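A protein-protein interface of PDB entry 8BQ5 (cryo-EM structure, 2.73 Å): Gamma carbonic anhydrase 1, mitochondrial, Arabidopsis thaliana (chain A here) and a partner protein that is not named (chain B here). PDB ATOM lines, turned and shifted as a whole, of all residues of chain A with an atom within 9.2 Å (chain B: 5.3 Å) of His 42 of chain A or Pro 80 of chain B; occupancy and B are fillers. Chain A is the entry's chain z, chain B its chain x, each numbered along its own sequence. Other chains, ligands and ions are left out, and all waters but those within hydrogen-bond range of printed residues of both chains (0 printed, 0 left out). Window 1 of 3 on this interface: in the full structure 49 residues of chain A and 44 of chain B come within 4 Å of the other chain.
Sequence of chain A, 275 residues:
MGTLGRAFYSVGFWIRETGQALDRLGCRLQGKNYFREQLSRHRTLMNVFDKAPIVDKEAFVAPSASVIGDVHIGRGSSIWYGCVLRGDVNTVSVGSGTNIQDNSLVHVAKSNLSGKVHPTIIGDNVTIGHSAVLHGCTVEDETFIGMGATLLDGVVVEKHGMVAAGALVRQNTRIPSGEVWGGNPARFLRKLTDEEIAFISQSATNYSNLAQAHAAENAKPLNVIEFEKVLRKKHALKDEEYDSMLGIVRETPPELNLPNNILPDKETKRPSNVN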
ATOM      1  N   LEU A  39      11.286  -9.734  -0.574  1.00  0.00           N
ATOM      2  CA  LEU A  39      11.074  -9.015   0.672  1.00  0.00           C
ATOM      3  C   LEU A  39      10.452  -9.956   1.692  1.00  0.00           C
ATOM      4  O   LEU A  39       9.691 -10.858   1.334  1.00  0.00           O
ATOM      5  CB  LEU A  39      10.179  -7.793   0.461  1.00  0.00           C
ATOM      6  CG  LEU A  39      10.677  -6.775  -0.565  1.00  0.00           C
ATOM      7  CD1 LEU A  39       9.512  -6.115  -1.282  1.00  0.00           C
ATOM      8  CD2 LEU A  39      11.559  -5.738   0.102  1.00  0.00           C
ATOM      9  N   SER A  40      10.787  -9.746   2.961  1.00  0.00           N
ATOM     10  CA  SER A  40      10.358 -10.670   4.002  1.00  0.00           C
ATOM     11  C   SER A  40       8.848 -10.625   4.183  1.00  0.00           C
ATOM     12  O   SER A  40       8.256  -9.554   4.341  1.00  0.00           O
ATOM     13  CB  SER A  40      11.054 -10.345   5.320  1.00  0.00           C
ATOM     14  OG  SER A  40      10.584 -11.199   6.347  1.00  0.00           O
ATOM     15  N   ARG A  41       8.231 -11.802   4.174  1.00  0.00           N
ATOM     16  CA  ARG A  41       6.799 -11.955   4.383  1.00  0.00           C
ATOM     17  C   ARG A  41       6.463 -12.226   5.843  1.00  0.00           C
ATOM     18  O   ARG A  41       5.338 -12.636   6.146  1.00  0.00           O
ATOM     19  CB  ARG A  41       6.266 -13.076   3.487  1.00  0.00           C
ATOM     20  CG  ARG A  41       6.927 -13.084   2.116  1.00  0.00           C
ATOM     21  CD  ARG A  41       6.083 -13.699   1.006  1.00  0.00           C
ATOM     22  NE  ARG A  41       4.648 -13.486   1.141  1.00  0.00           N
ATOM     23  CZ  ARG A  41       3.747 -14.007   0.321  1.00  0.00           C
ATOM     24  NH1 ARG A  41       4.104 -14.744  -0.718  1.00  0.00           N
ATOM     25  NH2 ARG A  41       2.456 -13.780   0.542  1.00  0.00           N
ATOM     26  N   HIS A  42       7.417 -12.017   6.749  1.00  0.00           N
ATOM     27  CA  HIS A  42       7.180 -12.250   8.166  1.00  0.00           C
ATOM     28  C   HIS A  42       6.174 -11.250   8.716  1.00  0.00           C
ATOM     29  O   HIS A  42       6.264 -10.048   8.454  1.00  0.00           O
ATOM     30  CB  HIS A  42       8.489 -12.149   8.951  1.00  0.00           C
ATOM     31  CG  HIS A  42       8.292 -11.985  10.427  1.00  0.00           C
ATOM     32  ND1 HIS A  42       7.912 -13.026  11.245  1.00  0.00           N
ATOM     33  CD2 HIS A  42       8.403 -10.900  11.226  1.00  0.00           C
ATOM     34  CE1 HIS A  42       7.808 -12.591  12.488  1.00  0.00           C
ATOM     35  NE2 HIS A  42       8.101 -11.303  12.504  1.00  0.00           N
ATOM     36  N   ARG A  43       5.227 -11.751   9.497  1.00  0.00           N
ATOM     37  CA  ARG A  43       4.247 -10.919  10.175  1.00  0.00           C
ATOM     38  C   ARG A  43       4.378 -11.139  11.674  1.00  0.00           C
ATOM     39  O   ARG A  43       4.368 -12.282  12.139  1.00  0.00           O
ATOM     40  CB  ARG A  43       2.828 -11.242   9.700  1.00  0.00           C
ATOM     41  CG  ARG A  43       2.448 -10.536   8.411  1.00  0.00           C
ATOM     42  CD  ARG A  43       1.087 -10.974   7.905  1.00  0.00           C
ATOM     43  NE  ARG A  43       1.067 -12.374   7.503  1.00  0.00           N
ATOM     44  CZ  ARG A  43      -0.038 -13.073   7.281  1.00  0.00           C
ATOM     45  NH1 ARG A  43      -1.237 -12.529   7.412  1.00  0.00           N
ATOM     46  NH2 ARG A  43       0.063 -14.347   6.914  1.00  0.00           N
ATOM     47  N   THR A  44       4.518 -10.042  12.421  1.00  0.00           N
ATOM     48  CA  THR A  44       4.587 -10.144  13.873  1.00  0.00           C
ATOM     49  C   THR A  44       3.320 -10.775  14.429  1.00  0.00           C
ATOM     50  O   THR A  44       3.381 -11.656  15.294  1.00  0.00           O
ATOM     51  CB  THR A  44       4.813  -8.760  14.483  1.00  0.00           C
ATOM     52  OG1 THR A  44       5.927  -8.128  13.840  1.00  0.00           O
ATOM     53  CG2 THR A  44       5.092  -8.867  15.967  1.00  0.00           C
ATOM     54  N   LEU A  45       2.167 -10.350  13.929  1.00  0.00           N
ATOM     55  CA  LEU A  45       0.878 -10.912  14.303  1.00  0.00           C
ATOM     56  C   LEU A  45       0.261 -11.565  13.075  1.00  0.00           C
ATOM     57  O   LEU A  45      -0.127 -10.870  12.131  1.00  0.00           O
ATOM     58  CB  LEU A  45      -0.048  -9.825  14.849  1.00  0.00           C
ATOM     59  CG  LEU A  45       0.429  -9.027  16.065  1.00  0.00           C
ATOM     60  CD1 LEU A  45      -0.749  -8.360  16.746  1.00  0.00           C
ATOM     61  CD2 LEU A  45       1.179  -9.904  17.051  1.00  0.00           C
ATOM     62  N   MET A  46       0.180 -12.891  13.082  1.00  0.00           N
ATOM     63  CA  MET A  46      -0.356 -13.629  11.947  1.00  0.00           C
ATOM     64  C   MET A  46      -1.631 -14.345  12.355  1.00  0.00           C
ATOM     65  O   MET A  46      -1.717 -14.894  13.458  1.00  0.00           O
ATOM     66  CB  MET A  46       0.656 -14.634  11.391  1.00  0.00           C
ATOM     67  CG  MET A  46       0.216 -15.207  10.052  1.00  0.00           C
ATOM     68  SD  MET A  46       0.616 -16.938   9.768  1.00  0.00           S
ATOM     69  CE  MET A  46       2.398 -16.870   9.789  1.00  0.00           C
ATOM     70  N   VAL A  61       5.625  -6.023  21.982  1.00  0.00           N
ATOM     71  CA  VAL A  61       5.963  -7.187  21.174  1.00  0.00           C
ATOM     72  C   VAL A  61       7.126  -6.793  20.277  1.00  0.00           C
ATOM     73  O   VAL A  61       7.046  -5.787  19.563  1.00  0.00           O
ATOM     74  CB  VAL A  61       4.773  -7.681  20.336  1.00  0.00           C
ATOM     75  CG1 VAL A  61       5.136  -8.956  19.598  1.00  0.00           C
ATOM     76  CG2 VAL A  61       3.553  -7.894  21.214  1.00  0.00           C
ATOM     77  N   ALA A  62       8.202  -7.567  20.324  1.00  0.00           N
ATOM     78  CA  ALA A  62       9.339  -7.292  19.460  1.00  0.00           C
ATOM     79  C   ALA A  62       8.957  -7.550  18.004  1.00  0.00           C
ATOM     80  O   ALA A  62       8.226  -8.504  17.715  1.00  0.00           O
ATOM     81  CB  ALA A  62      10.537  -8.155  19.855  1.00  0.00           C
ATOM     82  N   PRO A  63       9.426  -6.723  17.067  1.00  0.00           N
ATOM     83  CA  PRO A  63       9.021  -6.912  15.663  1.00  0.00           C
ATOM     84  C   PRO A  63       9.383  -8.276  15.103  1.00  0.00           C
ATOM     85  O   PRO A  63       8.668  -8.789  14.234  1.00  0.00           O
ATOM     86  CB  PRO A  63       9.753  -5.777  14.933  1.00  0.00           C
ATOM     87  CG  PRO A  63      10.015  -4.755  15.981  1.00  0.00           C
ATOM     88  CD  PRO A  63      10.239  -5.509  17.254  1.00  0.00           C
ATOM     89  N   SER A  64      10.465  -8.888  15.584  1.00  0.00           N
ATOM     90  CA  SER A  64      10.883 -10.197  15.095  1.00  0.00           C
ATOM     91  C   SER A  64      10.165 -11.355  15.777  1.00  0.00           C
ATOM     92  O   SER A  64      10.375 -12.505  15.382  1.00  0.00           O
ATOM     93  CB  SER A  64      12.397 -10.360  15.263  1.00  0.00           C
ATOM     94  OG  SER A  64      12.769 -10.351  16.629  1.00  0.00           O
ATOM     95  N   ALA A  65       9.331 -11.091  16.779  1.00  0.00           N
ATOM     96  CA  ALA A  65       8.573 -12.155  17.420  1.00  0.00           C
ATOM     97  C   ALA A  65       7.485 -12.677  16.487  1.00  0.00           C
ATOM     98  O   ALA A  65       7.020 -11.978  15.584  1.00  0.00           O
ATOM     99  CB  ALA A  65       7.952 -11.660  18.726  1.00  0.00           C
ATOM    100  N   SER A  66       7.086 -13.927  16.708  1.00  0.00           N
ATOM    101  CA  SER A  66       6.045 -14.578  15.922  1.00  0.00           C
ATOM    102  C   SER A  66       4.882 -14.933  16.837  1.00  0.00           C
ATOM    103  O   SER A  66       5.017 -15.794  17.713  1.00  0.00           O
ATOM    104  CB  SER A  66       6.578 -15.834  15.229  1.00  0.00           C
ATOM    105  OG  SER A  66       7.633 -15.527  14.338  1.00  0.00           O
ATOM    106  N   VAL A  67       3.748 -14.275  16.630  1.00  0.00           N
ATOM    107  CA  VAL A  67       2.529 -14.542  17.380  1.00  0.00           C
ATOM    108  C   VAL A  67       1.495 -15.038  16.379  1.00  0.00           C
ATOM    109  O   VAL A  67       1.035 -14.275  15.520  1.00  0.00           O
ATOM    110  CB  VAL A  67       2.036 -13.298  18.130  1.00  0.00           C
ATOM    111  CG1 VAL A  67       0.902 -13.657  19.050  1.00  0.00           C
ATOM    112  CG2 VAL A  67       3.177 -12.676  18.920  1.00  0.00           C
ATOM    113  N   ILE A  68       1.124 -16.310  16.491  1.00  0.00           N
ATOM    114  CA  ILE A  68       0.320 -16.991  15.485  1.00  0.00           C
ATOM    115  C   ILE A  68      -0.972 -17.480  16.122  1.00  0.00           C
ATOM    116  O   ILE A  68      -0.941 -18.175  17.143  1.00  0.00           O
ATOM    117  CB  ILE A  68       1.082 -18.171  14.858  1.00  0.00           C
ATOM    118  CG1 ILE A  68       2.406 -17.701  14.261  1.00  0.00           C
ATOM    119  CG2 ILE A  68       0.226 -18.842  13.812  1.00  0.00           C
ATOM    120  CD1 ILE A  68       3.626 -18.190  15.018  1.00  0.00           C
ATOM    121  N   GLY A  82      12.770 -12.674  19.059  1.00  0.00           N
ATOM    122  CA  GLY A  82      12.889 -14.061  18.666  1.00  0.00           C
ATOM    123  C   GLY A  82      11.872 -15.004  19.271  1.00  0.00           C
ATOM    124  O   GLY A  82      11.937 -16.209  18.999  1.00  0.00           O
ATOM    125  N   CYS A  83      10.939 -14.509  20.078  1.00  0.00           N
ATOM    126  CA  CYS A  83       9.959 -15.379  20.709  1.00  0.00           C
ATOM    127  C   CYS A  83       8.937 -15.874  19.693  1.00  0.00           C
ATOM    128  O   CYS A  83       8.597 -15.184  18.730  1.00  0.00           O
ATOM    129  CB  CYS A  83       9.246 -14.652  21.846  1.00  0.00           C
ATOM    130  SG  CYS A  83      10.305 -14.243  23.235  1.00  0.00           S
ATOM    131  N   VAL A  84       8.449 -17.091  19.913  1.00  0.00           N
ATOM    132  CA  VAL A  84       7.457 -17.708  19.042  1.00  0.00           C
ATOM    133  C   VAL A  84       6.290 -18.182  19.896  1.00  0.00           C
ATOM    134  O   VAL A  84       6.481 -18.942  20.850  1.00  0.00           O
ATOM    135  CB  VAL A  84       8.053 -18.879  18.235  1.00  0.00           C
ATOM    136  CG1 VAL A  84       6.980 -19.539  17.395  1.00  0.00           C
ATOM    137  CG2 VAL A  84       9.194 -18.390  17.353  1.00  0.00           C
ATOM    138  N   LEU A  85       5.085 -17.733  19.551  1.00  0.00           N
ATOM    139  CA  LEU A  85       3.860 -18.134  20.233  1.00  0.00           C
ATOM    140  C   LEU A  85       2.867 -18.626  19.192  1.00  0.00           C
ATOM    141  O   LEU A  85       2.414 -17.843  18.351  1.00  0.00           O
ATOM    142  CB  LEU A  85       3.268 -16.973  21.039  1.00  0.00           C
ATOM    143  CG  LEU A  85       4.067 -16.474  22.244  1.00  0.00           C
ATOM    144  CD1 LEU A  85       5.074 -15.422  21.826  1.00  0.00           C
ATOM    145  CD2 LEU A  85       3.136 -15.917  23.305  1.00  0.00           C
ATOM    146  N   GLN B  61      14.931 -15.092   2.879  1.00  0.00           N
ATOM    147  CA  GLN B  61      14.662 -16.463   3.297  1.00  0.00           C
ATOM    148  C   GLN B  61      15.612 -17.450   2.630  1.00  0.00           C
ATOM    149  O   GLN B  61      16.137 -18.356   3.287  1.00  0.00           O
ATOM    150  CB  GLN B  61      13.211 -16.826   2.992  1.00  0.00           C
ATOM    151  CG  GLN B  61      12.810 -18.211   3.459  1.00  0.00           C
ATOM    152  CD  GLN B  61      11.416 -18.592   3.015  1.00  0.00           C
ATOM    153  OE1 GLN B  61      11.139 -18.695   1.822  1.00  0.00           O
ATOM    154  NE2 GLN B  61      10.526 -18.794   3.976  1.00  0.00           N
ATOM    155  N   TYR B  77       5.809 -26.410   2.954  1.00  0.00           N
ATOM    156  CA  TYR B  77       5.591 -25.187   3.714  1.00  0.00           C
ATOM    157  C   TYR B  77       6.883 -24.776   4.409  1.00  0.00           C
ATOM    158  O   TYR B  77       7.461 -25.559   5.168  1.00  0.00           O
ATOM    159  CB  TYR B  77       4.476 -25.353   4.744  1.00  0.00           C
ATOM    160  CG  TYR B  77       4.319 -24.116   5.591  1.00  0.00           C
ATOM    161  CD1 TYR B  77       3.934 -22.912   5.022  1.00  0.00           C
ATOM    162  CD2 TYR B  77       4.603 -24.139   6.948  1.00  0.00           C
ATOM    163  CE1 TYR B  77       3.810 -21.772   5.784  1.00  0.00           C
ATOM    164  CE2 TYR B  77       4.483 -23.003   7.718  1.00  0.00           C
ATOM    165  CZ  TYR B  77       4.086 -21.823   7.131  1.00  0.00           C
ATOM    166  OH  TYR B  77       3.961 -20.686   7.893  1.00  0.00           O
ATOM    167  N   VAL B  78       7.325 -23.550   4.153  1.00  0.00           N
ATOM    168  CA  VAL B  78       8.473 -22.958   4.830  1.00  0.00           C
ATOM    169  C   VAL B  78       8.015 -21.636   5.429  1.00  0.00           C
ATOM    170  O   VAL B  78       7.554 -20.749   4.701  1.00  0.00           O
ATOM    171  CB  VAL B  78       9.662 -22.759   3.879  1.00  0.00           C
ATOM    172  CG1 VAL B  78      10.839 -22.147   4.616  1.00  0.00           C
ATOM    173  CG2 VAL B  78      10.062 -24.083   3.250  1.00  0.00           C
ATOM    174  N   ALA B  79       8.149 -21.505   6.746  1.00  0.00           N
ATOM    175  CA  ALA B  79       7.683 -20.313   7.435  1.00  0.00           C
ATOM    176  C   ALA B  79       8.440 -19.081   6.940  1.00  0.00           C
ATOM    177  O   ALA B  79       9.600 -19.180   6.530  1.00  0.00           O
ATOM    178  CB  ALA B  79       7.854 -20.465   8.944  1.00  0.00           C
ATOM    179  N   PRO B  80       7.799 -17.909   6.955  1.00  0.00           N
ATOM    180  CA  PRO B  80       8.432 -16.718   6.357  1.00  0.00           C
ATOM    181  C   PRO B  80       9.781 -16.348   6.957  1.00  0.00           C
ATOM    182  O   PRO B  80      10.672 -15.912   6.219  1.00  0.00           O
ATOM    183  CB  PRO B  80       7.387 -15.620   6.595  1.00  0.00           C
ATOM    184  CG  PRO B  80       6.097 -16.348   6.696  1.00  0.00           C
ATOM    185  CD  PRO B  80       6.415 -17.641   7.381  1.00  0.00           C
ATOM    186  N   ASN B  81       9.971 -16.510   8.264  1.00  0.00           N
ATOM    187  CA  ASN B  81      11.203 -16.071   8.907  1.00  0.00           C
ATOM    188  C   ASN B  81      12.261 -17.169   8.986  1.00  0.00           C
ATOM    189  O   ASN B  81      13.286 -16.978   9.647  1.00  0.00           O
ATOM    190  CB  ASN B  81      10.904 -15.508  10.301  1.00  0.00           C
ATOM    191  CG  ASN B  81      10.440 -16.563  11.280  1.00  0.00           C
ATOM    192  OD1 ASN B  81       9.964 -17.628  10.890  1.00  0.00           O
ATOM    193  ND2 ASN B  81      10.566 -16.265  12.565  1.00  0.00           N
ATOM    194  N   VAL B  82      12.036 -18.303   8.324  1.00  0.00           N
ATOM    195  CA  VAL B  82      13.050 -19.344   8.227  1.00  0.00           C
ATOM    196  C   VAL B  82      14.185 -18.877   7.321  1.00  0.00           C
ATOM    197  O   VAL B  82      13.974 -18.130   6.359  1.00  0.00           O
ATOM    198  CB  VAL B  82      12.415 -20.646   7.702  1.00  0.00           C
ATOM    199  CG1 VAL B  82      13.473 -21.672   7.328  1.00  0.00           C
ATOM    200  CG2 VAL B  82      11.459 -21.219   8.725  1.00  0.00           C
ATOM    201  N   ASN B  98       8.568 -21.727  12.222  1.00  0.00           N
ATOM    202  CA  ASN B  98       9.098 -20.398  12.516  1.00  0.00           C
ATOM    203  C   ASN B  98      10.409 -20.445  13.284  1.00  0.00           C
ATOM    204  O   ASN B  98      10.552 -21.188  14.257  1.00  0.00           O
ATOM    205  CB  ASN B  98       8.074 -19.590  13.313  1.00  0.00           C
ATOM    206  CG  ASN B  98       6.810 -19.331  12.537  1.00  0.00           C
ATOM    207  OD1 ASN B  98       6.034 -20.245  12.267  1.00  0.00           O
ATOM    208  ND2 ASN B  98       6.595 -18.076  12.170  1.00  0.00           N
ATOM    209  N   PHE B 235      -0.798 -17.923   2.154  1.00  0.00           N
ATOM    210  CA  PHE B 235       0.133 -17.093   1.400  1.00  0.00           C
ATOM    211  C   PHE B 235      -0.134 -17.232  -0.091  1.00  0.00           C
ATOM    212  O   PHE B 235      -0.187 -18.348  -0.617  1.00  0.00           O
ATOM    213  CB  PHE B 235       1.582 -17.463   1.721  1.00  0.00           C
ATOM    214  CG  PHE B 235       1.983 -17.150   3.131  1.00  0.00           C
ATOM    215  CD1 PHE B 235       2.403 -15.879   3.481  1.00  0.00           C
ATOM    216  CD2 PHE B 235       1.927 -18.125   4.111  1.00  0.00           C
ATOM    217  CE1 PHE B 235       2.766 -15.589   4.780  1.00  0.00           C
ATOM    218  CE2 PHE B 235       2.289 -17.841   5.411  1.00  0.00           C
ATOM    219  CZ  PHE B 235       2.708 -16.572   5.747  1.00  0.00           C
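Among the printed residues, merely in contact across the chains: Ser 66 of chain A with Asn 98 of chain B, Ser 66 of chain A with Asn 81 of chain B, Arg 41 of chain A with Pro 80 of chain B, His 42 of chain A with Pro 80 of chain B, Arg 41 of chain A with Phe 235 of chain B and Arg 43 of chain A with Phe 235 of chain B.
Printed residues of chain B that touch a printed residue of chain A: Pro 80, Asn 81, Asn 98 and Phe 235. Among the printed residues, no Asp or Glu carboxylate lies within 4 Å of a Lys or Arg side-chain nitrogen of the other chain.
Of the printed residues of chain B, His 42 of chain A touches Pro 80 (3.6 Å). No residue of chain A comes within 4 Å of Ala 79 of chain B. Printed residues of chain B within 4 Å of Ser 66 of chain A: Asn 81 (3.5 Å) and Asn 98 (3.5 Å). Of the printed residues of chain A, Asn 81 of chain B touches Ser 66. Of the printed residues of chain B, Arg 41 of chain A touches Pro 80 and Phe 235. Printed residues of chain B within 4 Å of Arg 43 of chain A: Phe 235. The nearest printed residue of chain B that does not touch His 42 of chain A is Asn 81 of chain B (4.0004 Å). The nearest residue of chain A that does not touch Pro 80 of chain B is Ser 40 of chain A (4.7 Å). The nearest printed residue of chain A that does not touch Asn 81 of chain B is His 42 of chain A (4.0004 Å).
The backbone NH of Ser 66 of chain A sits at hydrogen-bond distance from the backbone carbonyl oxygen of Cys 83 of chain A (2.8 Å). N of Leu 85 of chain A sits at hydrogen-bond distance from O of Ser 66 of chain A. The side-chain hydroxyl of Ser 40 of chain A sits close to the backbone NH of His 42 of chain A (3.3 Å). NE2 of His 42 of chain A sits close to O of Ala 65 of chain A (3.3 Å). NE2 of His 42 of chain A is in hydrogen-bond range of O of Pro 63 of chain A, at 3.1 Å.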
